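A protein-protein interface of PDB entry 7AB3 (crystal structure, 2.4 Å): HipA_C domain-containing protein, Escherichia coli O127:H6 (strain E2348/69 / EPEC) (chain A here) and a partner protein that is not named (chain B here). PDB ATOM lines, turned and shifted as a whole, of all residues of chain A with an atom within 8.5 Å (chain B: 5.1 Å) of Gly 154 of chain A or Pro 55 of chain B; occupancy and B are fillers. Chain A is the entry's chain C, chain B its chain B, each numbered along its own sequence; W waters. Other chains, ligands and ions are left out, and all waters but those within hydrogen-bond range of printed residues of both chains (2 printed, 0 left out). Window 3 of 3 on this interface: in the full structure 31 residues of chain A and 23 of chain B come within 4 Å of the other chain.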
ATOM      1  N   GLU A 150     -28.204 -19.191 -27.032  1.00  0.00           N
ATOM      2  CA  GLU A 150     -28.394 -18.056 -26.153  1.00  0.00           C
ATOM      3  C   GLU A 150     -29.680 -17.301 -26.461  1.00  0.00           C
ATOM      4  O   GLU A 150     -30.134 -17.301 -27.602  1.00  0.00           O
ATOM      5  CB  GLU A 150     -27.170 -17.145 -26.124  1.00  0.00           C
ATOM      6  CG  GLU A 150     -26.994 -16.340 -27.387  1.00  0.00           C
ATOM      7  CD  GLU A 150     -25.938 -15.275 -27.234  1.00  0.00           C
ATOM      8  OE1 GLU A 150     -25.830 -14.699 -26.125  1.00  0.00           O
ATOM      9  OE2 GLU A 150     -25.219 -15.020 -28.225  1.00  0.00           O
ATOM     10  N   GLN A 151     -30.283 -16.678 -25.444  1.00  0.00           N
ATOM     11  CA  GLN A 151     -31.512 -15.900 -25.646  1.00  0.00           C
ATOM     12  C   GLN A 151     -31.181 -14.506 -26.160  1.00  0.00           C
ATOM     13  O   GLN A 151     -30.104 -13.990 -25.883  1.00  0.00           O
ATOM     14  CB  GLN A 151     -32.367 -15.845 -24.371  1.00  0.00           C
ATOM     15  CG  GLN A 151     -33.527 -16.813 -24.371  1.00  0.00           C
ATOM     16  CD  GLN A 151     -33.080 -18.232 -24.499  1.00  0.00           C
ATOM     17  OE1 GLN A 151     -33.397 -18.927 -25.464  1.00  0.00           O
ATOM     18  NE2 GLN A 151     -32.348 -18.697 -23.502  1.00  0.00           N
ATOM     19  N   LEU A 152     -32.102 -13.903 -26.916  1.00  0.00           N
ATOM     20  CA  LEU A 152     -31.911 -12.594 -27.546  1.00  0.00           C
ATOM     21  C   LEU A 152     -31.731 -11.425 -26.593  1.00  0.00           C
ATOM     22  O   LEU A 152     -31.048 -10.471 -26.963  1.00  0.00           O
ATOM     23  CB  LEU A 152     -33.035 -12.286 -28.543  1.00  0.00           C
ATOM     24  CG  LEU A 152     -32.673 -12.488 -30.006  1.00  0.00           C
ATOM     25  CD1 LEU A 152     -31.633 -11.484 -30.450  1.00  0.00           C
ATOM     26  CD2 LEU A 152     -32.184 -13.913 -30.274  1.00  0.00           C
ATOM     27  N   ASP A 153     -32.298 -11.481 -25.376  1.00  0.00           N
ATOM     28  CA  ASP A 153     -32.121 -10.388 -24.417  1.00  0.00           C
ATOM     29  C   ASP A 153     -30.639 -10.238 -23.994  1.00  0.00           C
ATOM     30  O   ASP A 153     -30.127  -9.135 -23.987  1.00  0.00           O
ATOM     31  CB  ASP A 153     -33.088 -10.489 -23.220  1.00  0.00           C
ATOM     32  CG  ASP A 153     -32.882 -11.675 -22.305  1.00  0.00           C
ATOM     33  OD1 ASP A 153     -32.347 -12.696 -22.768  1.00  0.00           O
ATOM     34  OD2 ASP A 153     -33.254 -11.577 -21.120  1.00  0.00           O
ATOM     35  N   GLY A 154     -29.955 -11.343 -23.732  1.00  0.00           N
ATOM     36  CA  GLY A 154     -28.544 -11.336 -23.379  1.00  0.00           C
ATOM     37  C   GLY A 154     -27.640 -11.011 -24.555  1.00  0.00           C
ATOM     38  O   GLY A 154     -26.643 -10.319 -24.385  1.00  0.00           O
ATOM     39  N   ALA A 155     -28.000 -11.459 -25.762  1.00  0.00           N
ATOM     40  CA  ALA A 155     -27.242 -11.195 -26.984  1.00  0.00           C
ATOM     41  C   ALA A 155     -27.252  -9.690 -27.335  1.00  0.00           C
ATOM     42  O   ALA A 155     -26.194  -9.109 -27.624  1.00  0.00           O
ATOM     43  CB  ALA A 155     -27.810 -12.023 -28.135  1.00  0.00           C
ATOM     44  N   MET A 156     -28.434  -9.058 -27.268  1.00  0.00           N
ATOM     45  CA  MET A 156     -28.618  -7.628 -27.524  1.00  0.00           C
ATOM     46  C   MET A 156     -28.228  -6.750 -26.329  1.00  0.00           C
ATOM     47  O   MET A 156     -28.220  -5.523 -26.464  1.00  0.00           O
ATOM     48  CB  MET A 156     -30.081  -7.339 -27.889  1.00  0.00           C
ATOM     49  CG  MET A 156     -30.595  -8.142 -29.055  1.00  0.00           C
ATOM     50  SD  MET A 156     -32.284  -7.695 -29.530  1.00  0.00           S
ATOM     51  CE  MET A 156     -32.021  -6.036 -30.145  1.00  0.00           C
ATOM     52  N   GLN A 157     -27.916  -7.364 -25.168  1.00  0.00           N
ATOM     53  CA  GLN A 157     -27.517  -6.708 -23.927  1.00  0.00           C
ATOM     54  C   GLN A 157     -28.622  -5.859 -23.324  1.00  0.00           C
ATOM     55  O   GLN A 157     -28.367  -4.759 -22.827  1.00  0.00           O
ATOM     56  CB  GLN A 157     -26.226  -5.922 -24.103  1.00  0.00           C
ATOM     57  CG  GLN A 157     -25.086  -6.818 -24.497  1.00  0.00           C
ATOM     58  CD  GLN A 157     -23.843  -6.011 -24.705  1.00  0.00           C
ATOM     59  OE1 GLN A 157     -23.702  -5.343 -25.726  1.00  0.00           O
ATOM     60  NE2 GLN A 157     -22.933  -6.034 -23.740  1.00  0.00           N
ATOM     61  N   ILE A 158     -29.854  -6.392 -23.363  1.00  0.00           N
ATOM     62  CA  ILE A 158     -31.069  -5.804 -22.807  1.00  0.00           C
ATOM     63  C   ILE A 158     -31.288  -6.469 -21.445  1.00  0.00           C
ATOM     64  O   ILE A 158     -31.201  -7.687 -21.323  1.00  0.00           O
ATOM     65  CB  ILE A 158     -32.300  -5.968 -23.733  1.00  0.00           C
ATOM     66  CG1 ILE A 158     -31.967  -5.716 -25.210  1.00  0.00           C
ATOM     67  CG2 ILE A 158     -33.430  -5.073 -23.292  1.00  0.00           C
ATOM     68  CD1 ILE A 158     -31.468  -4.326 -25.536  1.00  0.00           C
ATOM     69  N   THR A 159     -31.524  -5.667 -20.410  1.00  0.00           N
ATOM     70  CA  THR A 159     -31.690  -6.155 -19.041  1.00  0.00           C
ATOM     71  C   THR A 159     -33.121  -6.623 -18.692  1.00  0.00           C
ATOM     72  O   THR A 159     -33.311  -7.289 -17.666  1.00  0.00           O
ATOM     73  CB  THR A 159     -31.196  -5.094 -18.093  1.00  0.00           C
ATOM     74  OG1 THR A 159     -31.932  -3.885 -18.336  1.00  0.00           O
ATOM     75  CG2 THR A 159     -29.700  -4.835 -18.271  1.00  0.00           C
ATOM     76  N   ASP A 160     -34.120  -6.281 -19.530  1.00  0.00           N
ATOM     77  CA  ASP A 160     -35.508  -6.692 -19.328  1.00  0.00           C
ATOM     78  C   ASP A 160     -35.971  -7.412 -20.602  1.00  0.00           C
ATOM     79  O   ASP A 160     -35.605  -6.991 -21.696  1.00  0.00           O
ATOM     80  CB  ASP A 160     -36.390  -5.458 -19.014  1.00  0.00           C
ATOM     81  CG  ASP A 160     -37.869  -5.747 -18.751  1.00  0.00           C
ATOM     82  OD1 ASP A 160     -38.192  -6.287 -17.668  1.00  0.00           O
ATOM     83  OD2 ASP A 160     -38.702  -5.419 -19.620  1.00  0.00           O
ATOM     84  N   LYS A 161     -36.770  -8.494 -20.477  1.00  0.00           N
ATOM     85  CA  LYS A 161     -37.220  -9.240 -21.663  1.00  0.00           C
ATOM     86  C   LYS A 161     -38.258  -8.501 -22.511  1.00  0.00           C
ATOM     87  O   LYS A 161     -38.481  -8.890 -23.646  1.00  0.00           O
ATOM     88  CB  LYS A 161     -37.700 -10.644 -21.307  1.00  0.00           C
ATOM     89  CG  LYS A 161     -38.856 -10.695 -20.334  1.00  0.00           C
ATOM     90  CD  LYS A 161     -39.030 -12.089 -19.788  1.00  0.00           C
ATOM     91  CE  LYS A 161     -40.353 -12.250 -19.092  1.00  0.00           C
ATOM     92  NZ  LYS A 161     -40.485 -13.585 -18.459  1.00  0.00           N
ATOM     93  N   PHE A 181     -31.089  -6.566 -35.711  1.00  0.00           N
ATOM     94  CA  PHE A 181     -30.014  -7.168 -34.933  1.00  0.00           C
ATOM     95  C   PHE A 181     -29.748  -8.602 -35.418  1.00  0.00           C
ATOM     96  O   PHE A 181     -28.599  -9.011 -35.508  1.00  0.00           O
ATOM     97  CB  PHE A 181     -30.392  -7.188 -33.433  1.00  0.00           C
ATOM     98  CG  PHE A 181     -29.363  -7.881 -32.570  1.00  0.00           C
ATOM     99  CD1 PHE A 181     -28.289  -7.184 -32.054  1.00  0.00           C
ATOM    100  CD2 PHE A 181     -29.448  -9.243 -32.317  1.00  0.00           C
ATOM    101  CE1 PHE A 181     -27.333  -7.822 -31.283  1.00  0.00           C
ATOM    102  CE2 PHE A 181     -28.476  -9.883 -31.567  1.00  0.00           C
ATOM    103  CZ  PHE A 181     -27.438  -9.160 -31.033  1.00  0.00           C
ATOM    104  N   LEU A 213     -38.180 -10.990 -25.758  1.00  0.00           N
ATOM    105  CA  LEU A 213     -36.783 -11.259 -26.086  1.00  0.00           C
ATOM    106  C   LEU A 213     -36.266 -12.593 -25.607  1.00  0.00           C
ATOM    107  O   LEU A 213     -35.351 -13.141 -26.225  1.00  0.00           O
ATOM    108  CB  LEU A 213     -35.884 -10.134 -25.576  1.00  0.00           C
ATOM    109  CG  LEU A 213     -36.108  -8.767 -26.195  1.00  0.00           C
ATOM    110  CD1 LEU A 213     -35.207  -7.753 -25.556  1.00  0.00           C
ATOM    111  CD2 LEU A 213     -35.908  -8.807 -27.705  1.00  0.00           C
ATOM    112  N   ARG A 214     -36.820 -13.128 -24.520  1.00  0.00           N
ATOM    113  CA  ARG A 214     -36.418 -14.465 -24.050  1.00  0.00           C
ATOM    114  C   ARG A 214     -37.110 -15.585 -24.858  1.00  0.00           C
ATOM    115  O   ARG A 214     -36.845 -16.752 -24.609  1.00  0.00           O
ATOM    116  CB  ARG A 214     -36.745 -14.646 -22.558  1.00  0.00           C
ATOM    117  CG  ARG A 214     -35.865 -13.855 -21.633  1.00  0.00           C
ATOM    118  CD  ARG A 214     -34.757 -14.713 -21.081  1.00  0.00           C
ATOM    119  NE  ARG A 214     -34.971 -15.057 -19.678  1.00  0.00           N
ATOM    120  CZ  ARG A 214     -34.629 -14.276 -18.650  1.00  0.00           C
ATOM    121  NH1 ARG A 214     -34.080 -13.084 -18.862  1.00  0.00           N
ATOM    122  NH2 ARG A 214     -34.841 -14.680 -17.404  1.00  0.00           N
ATOM    123  N   PHE A 216     -36.970 -15.725 -28.196  1.00  0.00           N
ATOM    124  CA  PHE A 216     -36.129 -15.755 -29.384  1.00  0.00           C
ATOM    125  C   PHE A 216     -34.777 -16.276 -28.920  1.00  0.00           C
ATOM    126  O   PHE A 216     -34.303 -15.913 -27.845  1.00  0.00           O
ATOM    127  CB  PHE A 216     -35.944 -14.368 -30.010  1.00  0.00           C
ATOM    128  CG  PHE A 216     -37.155 -13.810 -30.717  1.00  0.00           C
ATOM    129  CD1 PHE A 216     -37.354 -14.038 -32.065  1.00  0.00           C
ATOM    130  CD2 PHE A 216     -38.056 -12.995 -30.047  1.00  0.00           C
ATOM    131  CE1 PHE A 216     -38.458 -13.503 -32.720  1.00  0.00           C
ATOM    132  CE2 PHE A 216     -39.166 -12.481 -30.697  1.00  0.00           C
ATOM    133  CZ  PHE A 216     -39.353 -12.728 -32.032  1.00  0.00           C
ATOM    134  N   LEU A 218     -30.702 -18.067 -30.332  1.00  0.00           N
ATOM    135  CA  LEU A 218     -29.712 -18.302 -31.375  1.00  0.00           C
ATOM    136  C   LEU A 218     -29.083 -19.652 -31.119  1.00  0.00           C
ATOM    137  O   LEU A 218     -28.552 -19.857 -30.040  1.00  0.00           O
ATOM    138  CB  LEU A 218     -28.617 -17.228 -31.354  1.00  0.00           C
ATOM    139  CG  LEU A 218     -29.081 -15.842 -31.725  1.00  0.00           C
ATOM    140  CD1 LEU A 218     -27.949 -14.863 -31.595  1.00  0.00           C
ATOM    141  CD2 LEU A 218     -29.674 -15.825 -33.144  1.00  0.00           C
ATOM    142  N   SER B  38     -21.154 -15.871 -25.863  1.00  0.00           N
ATOM    143  CA  SER B  38     -22.236 -14.993 -26.255  1.00  0.00           C
ATOM    144  C   SER B  38     -21.756 -14.049 -27.351  1.00  0.00           C
ATOM    145  O   SER B  38     -20.574 -13.701 -27.376  1.00  0.00           O
ATOM    146  CB  SER B  38     -22.665 -14.169 -25.044  1.00  0.00           C
ATOM    147  OG  SER B  38     -23.617 -13.170 -25.367  1.00  0.00           O
ATOM    148  N   SER B  40     -22.469 -11.007 -27.291  1.00  0.00           N
ATOM    149  CA  SER B  40     -22.224  -9.833 -26.450  1.00  0.00           C
ATOM    150  C   SER B  40     -20.847  -9.879 -25.748  1.00  0.00           C
ATOM    151  O   SER B  40     -20.409  -8.873 -25.172  1.00  0.00           O
ATOM    152  CB  SER B  40     -23.326  -9.707 -25.403  1.00  0.00           C
ATOM    153  OG  SER B  40     -23.372 -10.823 -24.527  1.00  0.00           O
ATOM    154  N   LEU B  53     -24.320  -6.891 -13.213  1.00  0.00           N
ATOM    155  CA  LEU B  53     -24.049  -8.188 -13.830  1.00  0.00           C
ATOM    156  C   LEU B  53     -24.427  -8.162 -15.308  1.00  0.00           C
ATOM    157  O   LEU B  53     -25.556  -7.797 -15.649  1.00  0.00           O
ATOM    158  CB  LEU B  53     -24.798  -9.319 -13.108  1.00  0.00           C
ATOM    159  CG  LEU B  53     -24.542 -10.711 -13.656  1.00  0.00           C
ATOM    160  CD1 LEU B  53     -23.101 -11.115 -13.464  1.00  0.00           C
ATOM    161  CD2 LEU B  53     -25.459 -11.715 -13.029  1.00  0.00           C
ATOM    162  N   HIS B  54     -23.461  -8.536 -16.175  1.00  0.00           N
ATOM    163  CA  HIS B  54     -23.540  -8.599 -17.640  1.00  0.00           C
ATOM    164  C   HIS B  54     -24.865  -9.186 -18.113  1.00  0.00           C
ATOM    165  O   HIS B  54     -25.328 -10.183 -17.556  1.00  0.00           O
ATOM    166  CB  HIS B  54     -22.378  -9.440 -18.196  1.00  0.00           C
ATOM    167  CG  HIS B  54     -21.046  -9.109 -17.599  1.00  0.00           C
ATOM    168  ND1 HIS B  54     -20.743  -9.431 -16.278  1.00  0.00           N
ATOM    169  CD2 HIS B  54     -19.976  -8.492 -18.154  1.00  0.00           C
ATOM    170  CE1 HIS B  54     -19.512  -8.992 -16.077  1.00  0.00           C
ATOM    171  NE2 HIS B  54     -19.012  -8.419 -17.174  1.00  0.00           N
ATOM    172  N   PRO B  55     -25.493  -8.573 -19.133  1.00  0.00           N
ATOM    173  CA  PRO B  55     -26.801  -9.067 -19.610  1.00  0.00           C
ATOM    174  C   PRO B  55     -26.859 -10.554 -19.963  1.00  0.00           C
ATOM    175  O   PRO B  55     -27.918 -11.154 -19.841  1.00  0.00           O
ATOM    176  CB  PRO B  55     -27.093  -8.178 -20.824  1.00  0.00           C
ATOM    177  CG  PRO B  55     -26.329  -6.926 -20.554  1.00  0.00           C
ATOM    178  CD  PRO B  55     -25.067  -7.370 -19.873  1.00  0.00           C
ATOM    179  N   TYR B  56     -25.720 -11.150 -20.370  1.00  0.00           N
ATOM    180  CA  TYR B  56     -25.652 -12.568 -20.691  1.00  0.00           C
ATOM    181  C   TYR B  56     -25.809 -13.416 -19.433  1.00  0.00           C
ATOM    182  O   TYR B  56     -26.587 -14.364 -19.432  1.00  0.00           O
ATOM    183  CB  TYR B  56     -24.341 -12.916 -21.409  1.00  0.00           C
ATOM    184  CG  TYR B  56     -24.242 -14.389 -21.732  1.00  0.00           C
ATOM    185  CD1 TYR B  56     -25.097 -14.977 -22.652  1.00  0.00           C
ATOM    186  CD2 TYR B  56     -23.337 -15.209 -21.068  1.00  0.00           C
ATOM    187  CE1 TYR B  56     -25.038 -16.334 -22.931  1.00  0.00           C
ATOM    188  CE2 TYR B  56     -23.281 -16.575 -21.323  1.00  0.00           C
ATOM    189  CZ  TYR B  56     -24.136 -17.134 -22.260  1.00  0.00           C
ATOM    190  OH  TYR B  56     -24.086 -18.475 -22.545  1.00  0.00           O
ATOM    191  N   PHE B  57     -25.068 -13.084 -18.369  1.00  0.00           N
ATOM    192  CA  PHE B  57     -25.109 -13.815 -17.105  1.00  0.00           C
ATOM    193  C   PHE B  57     -26.407 -13.597 -16.333  1.00  0.00           C
ATOM    194  O   PHE B  57     -26.862 -14.499 -15.637  1.00  0.00           O
ATOM    195  CB  PHE B  57     -23.877 -13.488 -16.260  1.00  0.00           C
ATOM    196  CG  PHE B  57     -22.598 -13.930 -16.927  1.00  0.00           C
ATOM    197  CD1 PHE B  57     -22.258 -15.268 -16.989  1.00  0.00           C
ATOM    198  CD2 PHE B  57     -21.753 -13.009 -17.515  1.00  0.00           C
ATOM    199  CE1 PHE B  57     -21.087 -15.673 -17.610  1.00  0.00           C
ATOM    200  CE2 PHE B  57     -20.590 -13.416 -18.142  1.00  0.00           C
ATOM    201  CZ  PHE B  57     -20.264 -14.745 -18.185  1.00  0.00           C
ATOM    202  N   ALA B  58     -27.016 -12.418 -16.479  1.00  0.00           N
ATOM    203  CA  ALA B  58     -28.295 -12.124 -15.852  1.00  0.00           C
ATOM    204  C   ALA B  58     -29.424 -12.906 -16.573  1.00  0.00           C
ATOM    205  O   ALA B  58     -30.339 -13.397 -15.918  1.00  0.00           O
ATOM    206  CB  ALA B  58     -28.557 -10.627 -15.900  1.00  0.00           C
ATOM    207  N   SER B  59     -29.323 -13.062 -17.916  1.00  0.00           N
ATOM    208  CA  SER B  59     -30.275 -13.811 -18.755  1.00  0.00           C
ATOM    209  C   SER B  59     -30.228 -15.332 -18.485  1.00  0.00           C
ATOM    210  O   SER B  59     -31.186 -16.037 -18.793  1.00  0.00           O
ATOM    211  CB  SER B  59     -30.016 -13.533 -20.237  1.00  0.00           C
ATOM    212  OG  SER B  59     -30.636 -14.451 -21.128  1.00  0.00           O
HETATM  213  O   HOH W   1     -21.841  -7.822 -22.185  1.00  0.00           O
HETATM  214  O   HOH W   2     -28.186 -14.722 -23.350  1.00  0.00           O
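The side-chain carboxylate of Glu 150 of chain A lies within hydrogen-bond range of the side-chain hydroxyl of Ser 38 of chain B. The side-chain hydroxyl (OG) of Ser 40 of chain B is in hydrogen-bond range of the backbone carbonyl oxygen (O) of Gly 154 of chain A, 3.3 Å away. OG of Ser 59 of chain B lies within hydrogen-bond range of OD1 of Asp 153 of chain A (2.9 Å).
The side-chain hydroxyl (OG) of Ser 38 of chain B is in hydrogen-bond range of the side-chain hydroxyl (OG) of Ser 40 of chain B. The backbone carbonyl oxygen (O) of Glu 150 of chain A is in hydrogen-bond range of the backbone NH (N) of Leu 218 of chain A. The backbone carbonyl oxygen of Asp 153 of chain A is in hydrogen-bond range of the backbone NH of Ile 158 of chain A, 2.8 Å away. The side-chain carboxylate (OD2) of Asp 153 of chain A lies within salt-bridge range of the guanidinium group (NH1) of Arg 214 of chain A (2.8 Å).
CD1 of Tyr 56 of chain B touches OE1 of Glu 150 of chain A, at 3.6 Å. CB of Gln 151 of chain A touches OG of Ser 59 of chain B (3.9 Å). Gly 154 of chain A touches Pro 55 of chain B. Ala 155 of chain A touches Ser 40 of chain B. Gln 157 of chain A touches Ser 40 of chain B (CG to CB, 3.5 Å). Gln 157 of chain A touches Pro 55 of chain B. Ser 59 of chain B touches Arg 214 of chain A (O to CZ, 3.9 Å).
Of the printed residues of chain B, Gln 151 of chain A touches Ser 59 (3.9 Å). Gly 154 of chain A touches just these residues of chain B: Ser 40 and Pro 55. Of the printed residues of chain A, Ser 40 of chain B touches Gly 154 (3.3 Å), Ala 155 (3.7 Å) and Gln 157 (3.5 Å). Pro 55 of chain B touches two residues of chain A. Printed residues of chain A within 4 Å of Tyr 56 of chain B: Glu 150 (3.6 Å). The nearest printed residue of chain B that does not touch Gly 154 of chain A is Ser 59 of chain B (4.1 Å). The nearest residue of chain A that does not touch Pro 55 of chain B is Ile 158 of chain A (4.2 Å). The nearest printed residue of chain B that does not touch Ala 155 of chain A is Ser 38 of chain B (4.4 Å).
Of the 9 printed residues of chain B, 5 touch a printed residue of chain A. Printed residues of chain B that touch a printed residue of chain A: Ser 38, Ser 40, Pro 55, Tyr 56 and Ser 59. Hydrophobic or aromatic side chains of chain B that line the printed part of chain A: Pro 55 and Tyr 56. Among the printed residues, no Asp or Glu carboxylate lies within 4 Å of a Lys or Arg side-chain nitrogen of the other chain.
Water W1 lies within hydrogen-bond range of the side-chain amide nitrogen of Gln 157 of chain A (2.6 Å) and the backbone carbonyl oxygen of Ser 40 of chain B (3.5 Å). Water W2 lies within hydrogen-bond range of the backbone carbonyl oxygen of Gln 151 of chain A (3.3 Å) and the side-chain hydroxyl of Ser 59 of chain B (3.3 Å).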
